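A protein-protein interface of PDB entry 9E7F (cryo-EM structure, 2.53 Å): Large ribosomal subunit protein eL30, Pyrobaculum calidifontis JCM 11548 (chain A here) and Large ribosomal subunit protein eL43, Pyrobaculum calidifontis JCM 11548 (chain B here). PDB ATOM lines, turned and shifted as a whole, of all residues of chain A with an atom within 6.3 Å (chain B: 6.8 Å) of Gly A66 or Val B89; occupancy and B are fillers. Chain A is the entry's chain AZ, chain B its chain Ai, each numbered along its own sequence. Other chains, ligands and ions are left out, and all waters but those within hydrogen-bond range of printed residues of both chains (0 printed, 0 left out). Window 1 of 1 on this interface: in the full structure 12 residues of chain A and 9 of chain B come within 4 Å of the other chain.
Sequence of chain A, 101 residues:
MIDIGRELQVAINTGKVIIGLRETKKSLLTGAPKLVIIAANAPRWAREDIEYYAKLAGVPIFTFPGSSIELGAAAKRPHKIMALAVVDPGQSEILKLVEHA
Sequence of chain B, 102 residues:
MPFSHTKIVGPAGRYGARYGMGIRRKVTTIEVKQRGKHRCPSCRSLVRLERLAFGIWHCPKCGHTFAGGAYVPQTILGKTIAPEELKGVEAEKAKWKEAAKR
The backbone carbonyl oxygen of Ser B42 lies within hydrogen-bond range of the side-chain amide nitrogen of Asn A41, 3.2 Å away.
The side-chain carboxylate (OE1) of Glu A70 is in salt-bridge range of the side-chain amino group (NZ) of Lys B93, 3.5 Å away.
O of Gly B88 touches CB of Ala A40 (3.9 Å).
CB of Ala A40 touches CG2 of Val B89, 3.6 Å away.
Asn A41 touches Arg B44 (ND2 to CG, 3.7 Å).
CB of Asn A41 touches CG2 of Val B89, at 3.6 Å.
CG of Glu B92 touches CG2 of Thr A63 (3.7 Å).
O of Val B89 touches O of Pro A65 (3.8 Å).
CA of Pro A65 touches CG of Glu B92, at 3.9 Å.
Lys B93 touches Pro A65 (CE to O, 3.6 Å).
Val B89 touches Gly A66.
Val B89 touches Ser A67 (CG2 to CA, 3.8 Å).
Gly A66 touches just one residue of chain B: Val B89 (3.4 Å).
Of the printed residues of chain A, Ser B42 touches Asn A41.
Glu B85 touches none of the printed residues of chain A.
Of chain A, only Ala A40, Asn A41, Pro A65, Gly A66 and Ser A67 come within 4 Å of Val B89.
Printed residues of chain A within 4 Å of Lys B93: Pro A65 and Glu A70.
The backbone NH of Ala A40 lies within hydrogen-bond range of the backbone carbonyl oxygen of Gly A66, at 3.2 Å.
The backbone NH (N) of Ser A68 lies within hydrogen-bond range of the side-chain amide oxygen (OD1) of Asn A41, at 2.8 Å.
The side-chain hydroxyl (OG) of Ser A67 is in hydrogen-bond range of the backbone NH (N) of Ile A69 (3.1 Å).
The side-chain carboxylate (OE2) of Glu A70 sits at hydrogen-bond distance from the backbone NH (N) of Ser A67 (2.9 Å).
NH2 of Arg B44 is in hydrogen-bond range of O of Leu B86, at 3.1 Å.
The side-chain carboxylate (OE2) of Glu B90 is in salt-bridge range of the guanidinium group (NH1) of Arg B44 (3.7 Å).
Hydrophobic or aromatic side chains of chain A within 4 Å of the printed part of chain B: Ala A40 and Pro A65.
Among the printed residues, 12 pairs touch across the chains.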
ATOM      1  N   ILE A  38      -5.454  24.734  22.377  1.00  0.00           N
ATOM      2  CA  ILE A  38      -5.769  23.328  22.171  1.00  0.00           C
ATOM      3  C   ILE A  38      -4.471  22.535  22.167  1.00  0.00           C
ATOM      4  O   ILE A  38      -3.458  22.984  21.620  1.00  0.00           O
ATOM      5  CB  ILE A  38      -6.559  23.107  20.867  1.00  0.00           C
ATOM      6  CG1 ILE A  38      -7.113  21.687  20.824  1.00  0.00           C
ATOM      7  CG2 ILE A  38      -5.696  23.382  19.657  1.00  0.00           C
ATOM      8  CD1 ILE A  38      -8.010  21.427  19.660  1.00  0.00           C
ATOM      9  N   ALA A  39      -4.492  21.369  22.804  1.00  0.00           N
ATOM     10  CA  ALA A  39      -3.311  20.523  22.835  1.00  0.00           C
ATOM     11  C   ALA A  39      -3.008  19.975  21.446  1.00  0.00           C
ATOM     12  O   ALA A  39      -3.905  19.771  20.623  1.00  0.00           O
ATOM     13  CB  ALA A  39      -3.497  19.376  23.825  1.00  0.00           C
ATOM     14  N   ALA A  40      -1.720  19.740  21.190  1.00  0.00           N
ATOM     15  CA  ALA A  40      -1.298  19.297  19.867  1.00  0.00           C
ATOM     16  C   ALA A  40      -1.808  17.902  19.549  1.00  0.00           C
ATOM     17  O   ALA A  40      -2.107  17.602  18.388  1.00  0.00           O
ATOM     18  CB  ALA A  40       0.225  19.340  19.761  1.00  0.00           C
ATOM     19  N   ASN A  41      -1.921  17.035  20.554  1.00  0.00           N
ATOM     20  CA  ASN A  41      -2.369  15.665  20.351  1.00  0.00           C
ATOM     21  C   ASN A  41      -3.874  15.507  20.551  1.00  0.00           C
ATOM     22  O   ASN A  41      -4.343  14.425  20.915  1.00  0.00           O
ATOM     23  CB  ASN A  41      -1.598  14.716  21.267  1.00  0.00           C
ATOM     24  CG  ASN A  41      -1.985  14.863  22.716  1.00  0.00           C
ATOM     25  OD1 ASN A  41      -2.303  15.954  23.179  1.00  0.00           O
ATOM     26  ND2 ASN A  41      -1.971  13.756  23.442  1.00  0.00           N
ATOM     27  N   THR A  63      -2.100  26.420  19.176  1.00  0.00           N
ATOM     28  CA  THR A  63      -1.843  25.006  19.407  1.00  0.00           C
ATOM     29  C   THR A  63      -0.694  24.897  20.395  1.00  0.00           C
ATOM     30  O   THR A  63       0.419  25.348  20.111  1.00  0.00           O
ATOM     31  CB  THR A  63      -1.519  24.285  18.105  1.00  0.00           C
ATOM     32  OG1 THR A  63      -2.728  24.054  17.374  1.00  0.00           O
ATOM     33  CG2 THR A  63      -0.852  22.958  18.394  1.00  0.00           C
ATOM     34  N   PHE A  64      -0.970  24.322  21.557  1.00  0.00           N
ATOM     35  CA  PHE A  64       0.052  24.180  22.578  1.00  0.00           C
ATOM     36  C   PHE A  64       1.149  23.243  22.084  1.00  0.00           C
ATOM     37  O   PHE A  64       0.856  22.211  21.473  1.00  0.00           O
ATOM     38  CB  PHE A  64      -0.561  23.638  23.869  1.00  0.00           C
ATOM     39  CG  PHE A  64       0.371  23.660  25.034  1.00  0.00           C
ATOM     40  CD1 PHE A  64       0.751  24.855  25.606  1.00  0.00           C
ATOM     41  CD2 PHE A  64       0.859  22.484  25.566  1.00  0.00           C
ATOM     42  CE1 PHE A  64       1.611  24.874  26.682  1.00  0.00           C
ATOM     43  CE2 PHE A  64       1.720  22.496  26.636  1.00  0.00           C
ATOM     44  CZ  PHE A  64       2.094  23.692  27.197  1.00  0.00           C
ATOM     45  N   PRO A  65       2.418  23.559  22.338  1.00  0.00           N
ATOM     46  CA  PRO A  65       3.516  22.715  21.857  1.00  0.00           C
ATOM     47  C   PRO A  65       3.751  21.445  22.660  1.00  0.00           C
ATOM     48  O   PRO A  65       4.821  20.846  22.530  1.00  0.00           O
ATOM     49  CB  PRO A  65       4.733  23.650  21.942  1.00  0.00           C
ATOM     50  CG  PRO A  65       4.364  24.717  22.883  1.00  0.00           C
ATOM     51  CD  PRO A  65       2.884  24.790  22.995  1.00  0.00           C
ATOM     52  N   GLY A  66       2.804  21.023  23.491  1.00  0.00           N
ATOM     53  CA  GLY A  66       2.856  19.738  24.153  1.00  0.00           C
ATOM     54  C   GLY A  66       1.582  18.948  23.931  1.00  0.00           C
ATOM     55  O   GLY A  66       0.820  19.242  23.008  1.00  0.00           O
ATOM     56  N   SER A  67       1.340  17.949  24.761  1.00  0.00           N
ATOM     57  CA  SER A  67       0.144  17.138  24.671  1.00  0.00           C
ATOM     58  C   SER A  67      -0.912  17.667  25.635  1.00  0.00           C
ATOM     59  O   SER A  67      -0.752  18.722  26.252  1.00  0.00           O
ATOM     60  CB  SER A  67       0.475  15.679  24.962  1.00  0.00           C
ATOM     61  OG  SER A  67       0.603  15.471  26.352  1.00  0.00           O
ATOM     62  N   SER A  68      -2.013  16.926  25.757  1.00  0.00           N
ATOM     63  CA  SER A  68      -3.034  17.270  26.738  1.00  0.00           C
ATOM     64  C   SER A  68      -2.491  17.169  28.153  1.00  0.00           C
ATOM     65  O   SER A  68      -2.857  17.963  29.027  1.00  0.00           O
ATOM     66  CB  SER A  68      -4.238  16.355  26.570  1.00  0.00           C
ATOM     67  OG  SER A  68      -3.991  15.106  27.186  1.00  0.00           O
ATOM     68  N   ILE A  69      -1.628  16.187  28.403  1.00  0.00           N
ATOM     69  CA  ILE A  69      -1.065  16.018  29.737  1.00  0.00           C
ATOM     70  C   ILE A  69      -0.140  17.173  30.080  1.00  0.00           C
ATOM     71  O   ILE A  69      -0.228  17.754  31.167  1.00  0.00           O
ATOM     72  CB  ILE A  69      -0.339  14.668  29.841  1.00  0.00           C
ATOM     73  CG1 ILE A  69      -1.117  13.591  29.092  1.00  0.00           C
ATOM     74  CG2 ILE A  69      -0.165  14.280  31.290  1.00  0.00           C
ATOM     75  CD1 ILE A  69      -1.698  12.536  29.984  1.00  0.00           C
ATOM     76  N   GLU A  70       0.764  17.530  29.163  1.00  0.00           N
ATOM     77  CA  GLU A  70       1.709  18.602  29.455  1.00  0.00           C
ATOM     78  C   GLU A  70       1.012  19.954  29.498  1.00  0.00           C
ATOM     79  O   GLU A  70       1.472  20.871  30.185  1.00  0.00           O
ATOM     80  CB  GLU A  70       2.849  18.618  28.437  1.00  0.00           C
ATOM     81  CG  GLU A  70       3.232  17.259  27.882  1.00  0.00           C
ATOM     82  CD  GLU A  70       3.879  17.351  26.513  1.00  0.00           C
ATOM     83  OE1 GLU A  70       4.561  18.357  26.241  1.00  0.00           O
ATOM     84  OE2 GLU A  70       3.688  16.429  25.695  1.00  0.00           O
ATOM     85  N   LEU A  71      -0.090  20.100  28.761  1.00  0.00           N
ATOM     86  CA  LEU A  71      -0.891  21.313  28.870  1.00  0.00           C
ATOM     87  C   LEU A  71      -1.480  21.448  30.264  1.00  0.00           C
ATOM     88  O   LEU A  71      -1.488  22.540  30.839  1.00  0.00           O
ATOM     89  CB  LEU A  71      -1.994  21.309  27.815  1.00  0.00           C
ATOM     90  CG  LEU A  71      -3.030  22.429  27.901  1.00  0.00           C
ATOM     91  CD1 LEU A  71      -2.337  23.770  27.987  1.00  0.00           C
ATOM     92  CD2 LEU A  71      -3.981  22.393  26.720  1.00  0.00           C
ATOM     93  N   SER B  42      -1.545   7.757  20.919  1.00  0.00           N
ATOM     94  CA  SER B  42      -2.412   8.893  20.644  1.00  0.00           C
ATOM     95  C   SER B  42      -2.522   9.822  21.848  1.00  0.00           C
ATOM     96  O   SER B  42      -2.102  10.980  21.784  1.00  0.00           O
ATOM     97  CB  SER B  42      -3.795   8.395  20.231  1.00  0.00           C
ATOM     98  OG  SER B  42      -4.689   8.463  21.324  1.00  0.00           O
ATOM     99  N   ARG B  44      -1.130   9.461  24.906  1.00  0.00           N
ATOM    100  CA  ARG B  44       0.090   9.491  25.708  1.00  0.00           C
ATOM    101  C   ARG B  44      -0.146   9.172  27.178  1.00  0.00           C
ATOM    102  O   ARG B  44       0.698   9.496  28.015  1.00  0.00           O
ATOM    103  CB  ARG B  44       0.808  10.840  25.588  1.00  0.00           C
ATOM    104  CG  ARG B  44       0.794  11.425  24.193  1.00  0.00           C
ATOM    105  CD  ARG B  44       2.183  11.598  23.647  1.00  0.00           C
ATOM    106  NE  ARG B  44       2.177  11.648  22.193  1.00  0.00           N
ATOM    107  CZ  ARG B  44       3.172  12.121  21.457  1.00  0.00           C
ATOM    108  NH1 ARG B  44       4.272  12.603  22.011  1.00  0.00           N
ATOM    109  NH2 ARG B  44       3.062  12.112  20.133  1.00  0.00           N
ATOM    110  N   GLU B  85       0.829  11.482  11.525  1.00  0.00           N
ATOM    111  CA  GLU B  85      -0.376  12.082  12.082  1.00  0.00           C
ATOM    112  C   GLU B  85      -0.294  12.078  13.601  1.00  0.00           C
ATOM    113  O   GLU B  85      -0.735  13.032  14.250  1.00  0.00           O
ATOM    114  CB  GLU B  85      -1.614  11.340  11.535  1.00  0.00           C
ATOM    115  CG  GLU B  85      -3.072  11.634  12.060  1.00  0.00           C
ATOM    116  CD  GLU B  85      -3.386  11.296  13.517  1.00  0.00           C
ATOM    117  OE1 GLU B  85      -3.289  10.110  13.888  1.00  0.00           O
ATOM    118  OE2 GLU B  85      -3.720  12.221  14.285  1.00  0.00           O
ATOM    119  N   LEU B  86       0.243  11.009  14.185  1.00  0.00           N
ATOM    120  CA  LEU B  86       0.458  10.944  15.618  1.00  0.00           C
ATOM    121  C   LEU B  86       1.723  11.660  16.050  1.00  0.00           C
ATOM    122  O   LEU B  86       1.971  11.770  17.253  1.00  0.00           O
ATOM    123  CB  LEU B  86       0.525   9.489  16.088  1.00  0.00           C
ATOM    124  CG  LEU B  86      -0.654   8.596  15.719  1.00  0.00           C
ATOM    125  CD1 LEU B  86      -0.160   7.261  15.204  1.00  0.00           C
ATOM    126  CD2 LEU B  86      -1.565   8.408  16.908  1.00  0.00           C
ATOM    127  N   LYS B  87       2.537  12.117  15.109  1.00  0.00           N
ATOM    128  CA  LYS B  87       3.680  12.967  15.427  1.00  0.00           C
ATOM    129  C   LYS B  87       3.324  14.433  15.191  1.00  0.00           C
ATOM    130  O   LYS B  87       3.868  15.109  14.318  1.00  0.00           O
ATOM    131  CB  LYS B  87       4.897  12.549  14.610  1.00  0.00           C
ATOM    132  CG  LYS B  87       5.329  11.113  14.842  1.00  0.00           C
ATOM    133  CD  LYS B  87       5.368  10.787  16.324  1.00  0.00           C
ATOM    134  CE  LYS B  87       6.481  11.530  17.030  1.00  0.00           C
ATOM    135  NZ  LYS B  87       6.603  11.098  18.445  1.00  0.00           N
ATOM    136  N   GLY B  88       2.368  14.913  15.979  1.00  0.00           N
ATOM    137  CA  GLY B  88       1.959  16.299  15.918  1.00  0.00           C
ATOM    138  C   GLY B  88       2.469  17.091  17.102  1.00  0.00           C
ATOM    139  O   GLY B  88       2.739  18.290  16.989  1.00  0.00           O
ATOM    140  N   VAL B  89       2.596  16.427  18.250  1.00  0.00           N
ATOM    141  CA  VAL B  89       3.147  17.083  19.432  1.00  0.00           C
ATOM    142  C   VAL B  89       4.603  17.450  19.193  1.00  0.00           C
ATOM    143  O   VAL B  89       5.048  18.558  19.516  1.00  0.00           O
ATOM    144  CB  VAL B  89       2.995  16.182  20.668  1.00  0.00           C
ATOM    145  CG1 VAL B  89       4.099  16.473  21.664  1.00  0.00           C
ATOM    146  CG2 VAL B  89       1.639  16.386  21.302  1.00  0.00           C
ATOM    147  N   GLU B  90       5.364  16.521  18.622  1.00  0.00           N
ATOM    148  CA  GLU B  90       6.772  16.780  18.355  1.00  0.00           C
ATOM    149  C   GLU B  90       6.943  17.791  17.231  1.00  0.00           C
ATOM    150  O   GLU B  90       7.889  18.585  17.245  1.00  0.00           O
ATOM    151  CB  GLU B  90       7.482  15.470  18.026  1.00  0.00           C
ATOM    152  CG  GLU B  90       7.188  14.354  19.018  1.00  0.00           C
ATOM    153  CD  GLU B  90       8.045  14.449  20.267  1.00  0.00           C
ATOM    154  OE1 GLU B  90       9.060  15.176  20.234  1.00  0.00           O
ATOM    155  OE2 GLU B  90       7.706  13.800  21.280  1.00  0.00           O
ATOM    156  N   ALA B  91       6.045  17.771  16.245  1.00  0.00           N
ATOM    157  CA  ALA B  91       6.131  18.721  15.144  1.00  0.00           C
ATOM    158  C   ALA B  91       5.920  20.150  15.627  1.00  0.00           C
ATOM    159  O   ALA B  91       6.661  21.062  15.250  1.00  0.00           O
ATOM    160  CB  ALA B  91       5.109  18.365  14.067  1.00  0.00           C
ATOM    161  N   GLU B  92       4.910  20.362  16.471  1.00  0.00           N
ATOM    162  CA  GLU B  92       4.675  21.701  16.996  1.00  0.00           C
ATOM    163  C   GLU B  92       5.736  22.075  18.025  1.00  0.00           C
ATOM    164  O   GLU B  92       6.007  23.261  18.247  1.00  0.00           O
ATOM    165  CB  GLU B  92       3.273  21.787  17.598  1.00  0.00           C
ATOM    166  CG  GLU B  92       2.781  23.183  18.040  1.00  0.00           C
ATOM    167  CD  GLU B  92       3.410  24.381  17.308  1.00  0.00           C
ATOM    168  OE1 GLU B  92       3.607  25.428  17.962  1.00  0.00           O
ATOM    169  OE2 GLU B  92       3.652  24.314  16.083  1.00  0.00           O
ATOM    170  N   LYS B  93       6.345  21.076  18.669  1.00  0.00           N
ATOM    171  CA  LYS B  93       7.442  21.350  19.591  1.00  0.00           C
ATOM    172  C   LYS B  93       8.618  21.987  18.867  1.00  0.00           C
ATOM    173  O   LYS B  93       9.260  22.904  19.389  1.00  0.00           O
ATOM    174  CB  LYS B  93       7.884  20.064  20.288  1.00  0.00           C
ATOM    175  CG  LYS B  93       8.581  20.281  21.623  1.00  0.00           C
ATOM    176  CD  LYS B  93       8.543  19.034  22.488  1.00  0.00           C
ATOM    177  CE  LYS B  93       7.760  19.262  23.760  1.00  0.00           C
ATOM    178  NZ  LYS B  93       7.583  18.000  24.524  1.00  0.00           N
ATOM    179  N   ALA B  94       8.919  21.507  17.661  1.00  0.00           N
ATOM    180  CA  ALA B  94       9.962  22.127  16.853  1.00  0.00           C
ATOM    181  C   ALA B  94       9.577  23.546  16.465  1.00  0.00           C
ATOM    182  O   ALA B  94      10.393  24.470  16.547  1.00  0.00           O
ATOM    183  CB  ALA B  94      10.226  21.283  15.609  1.00  0.00           C
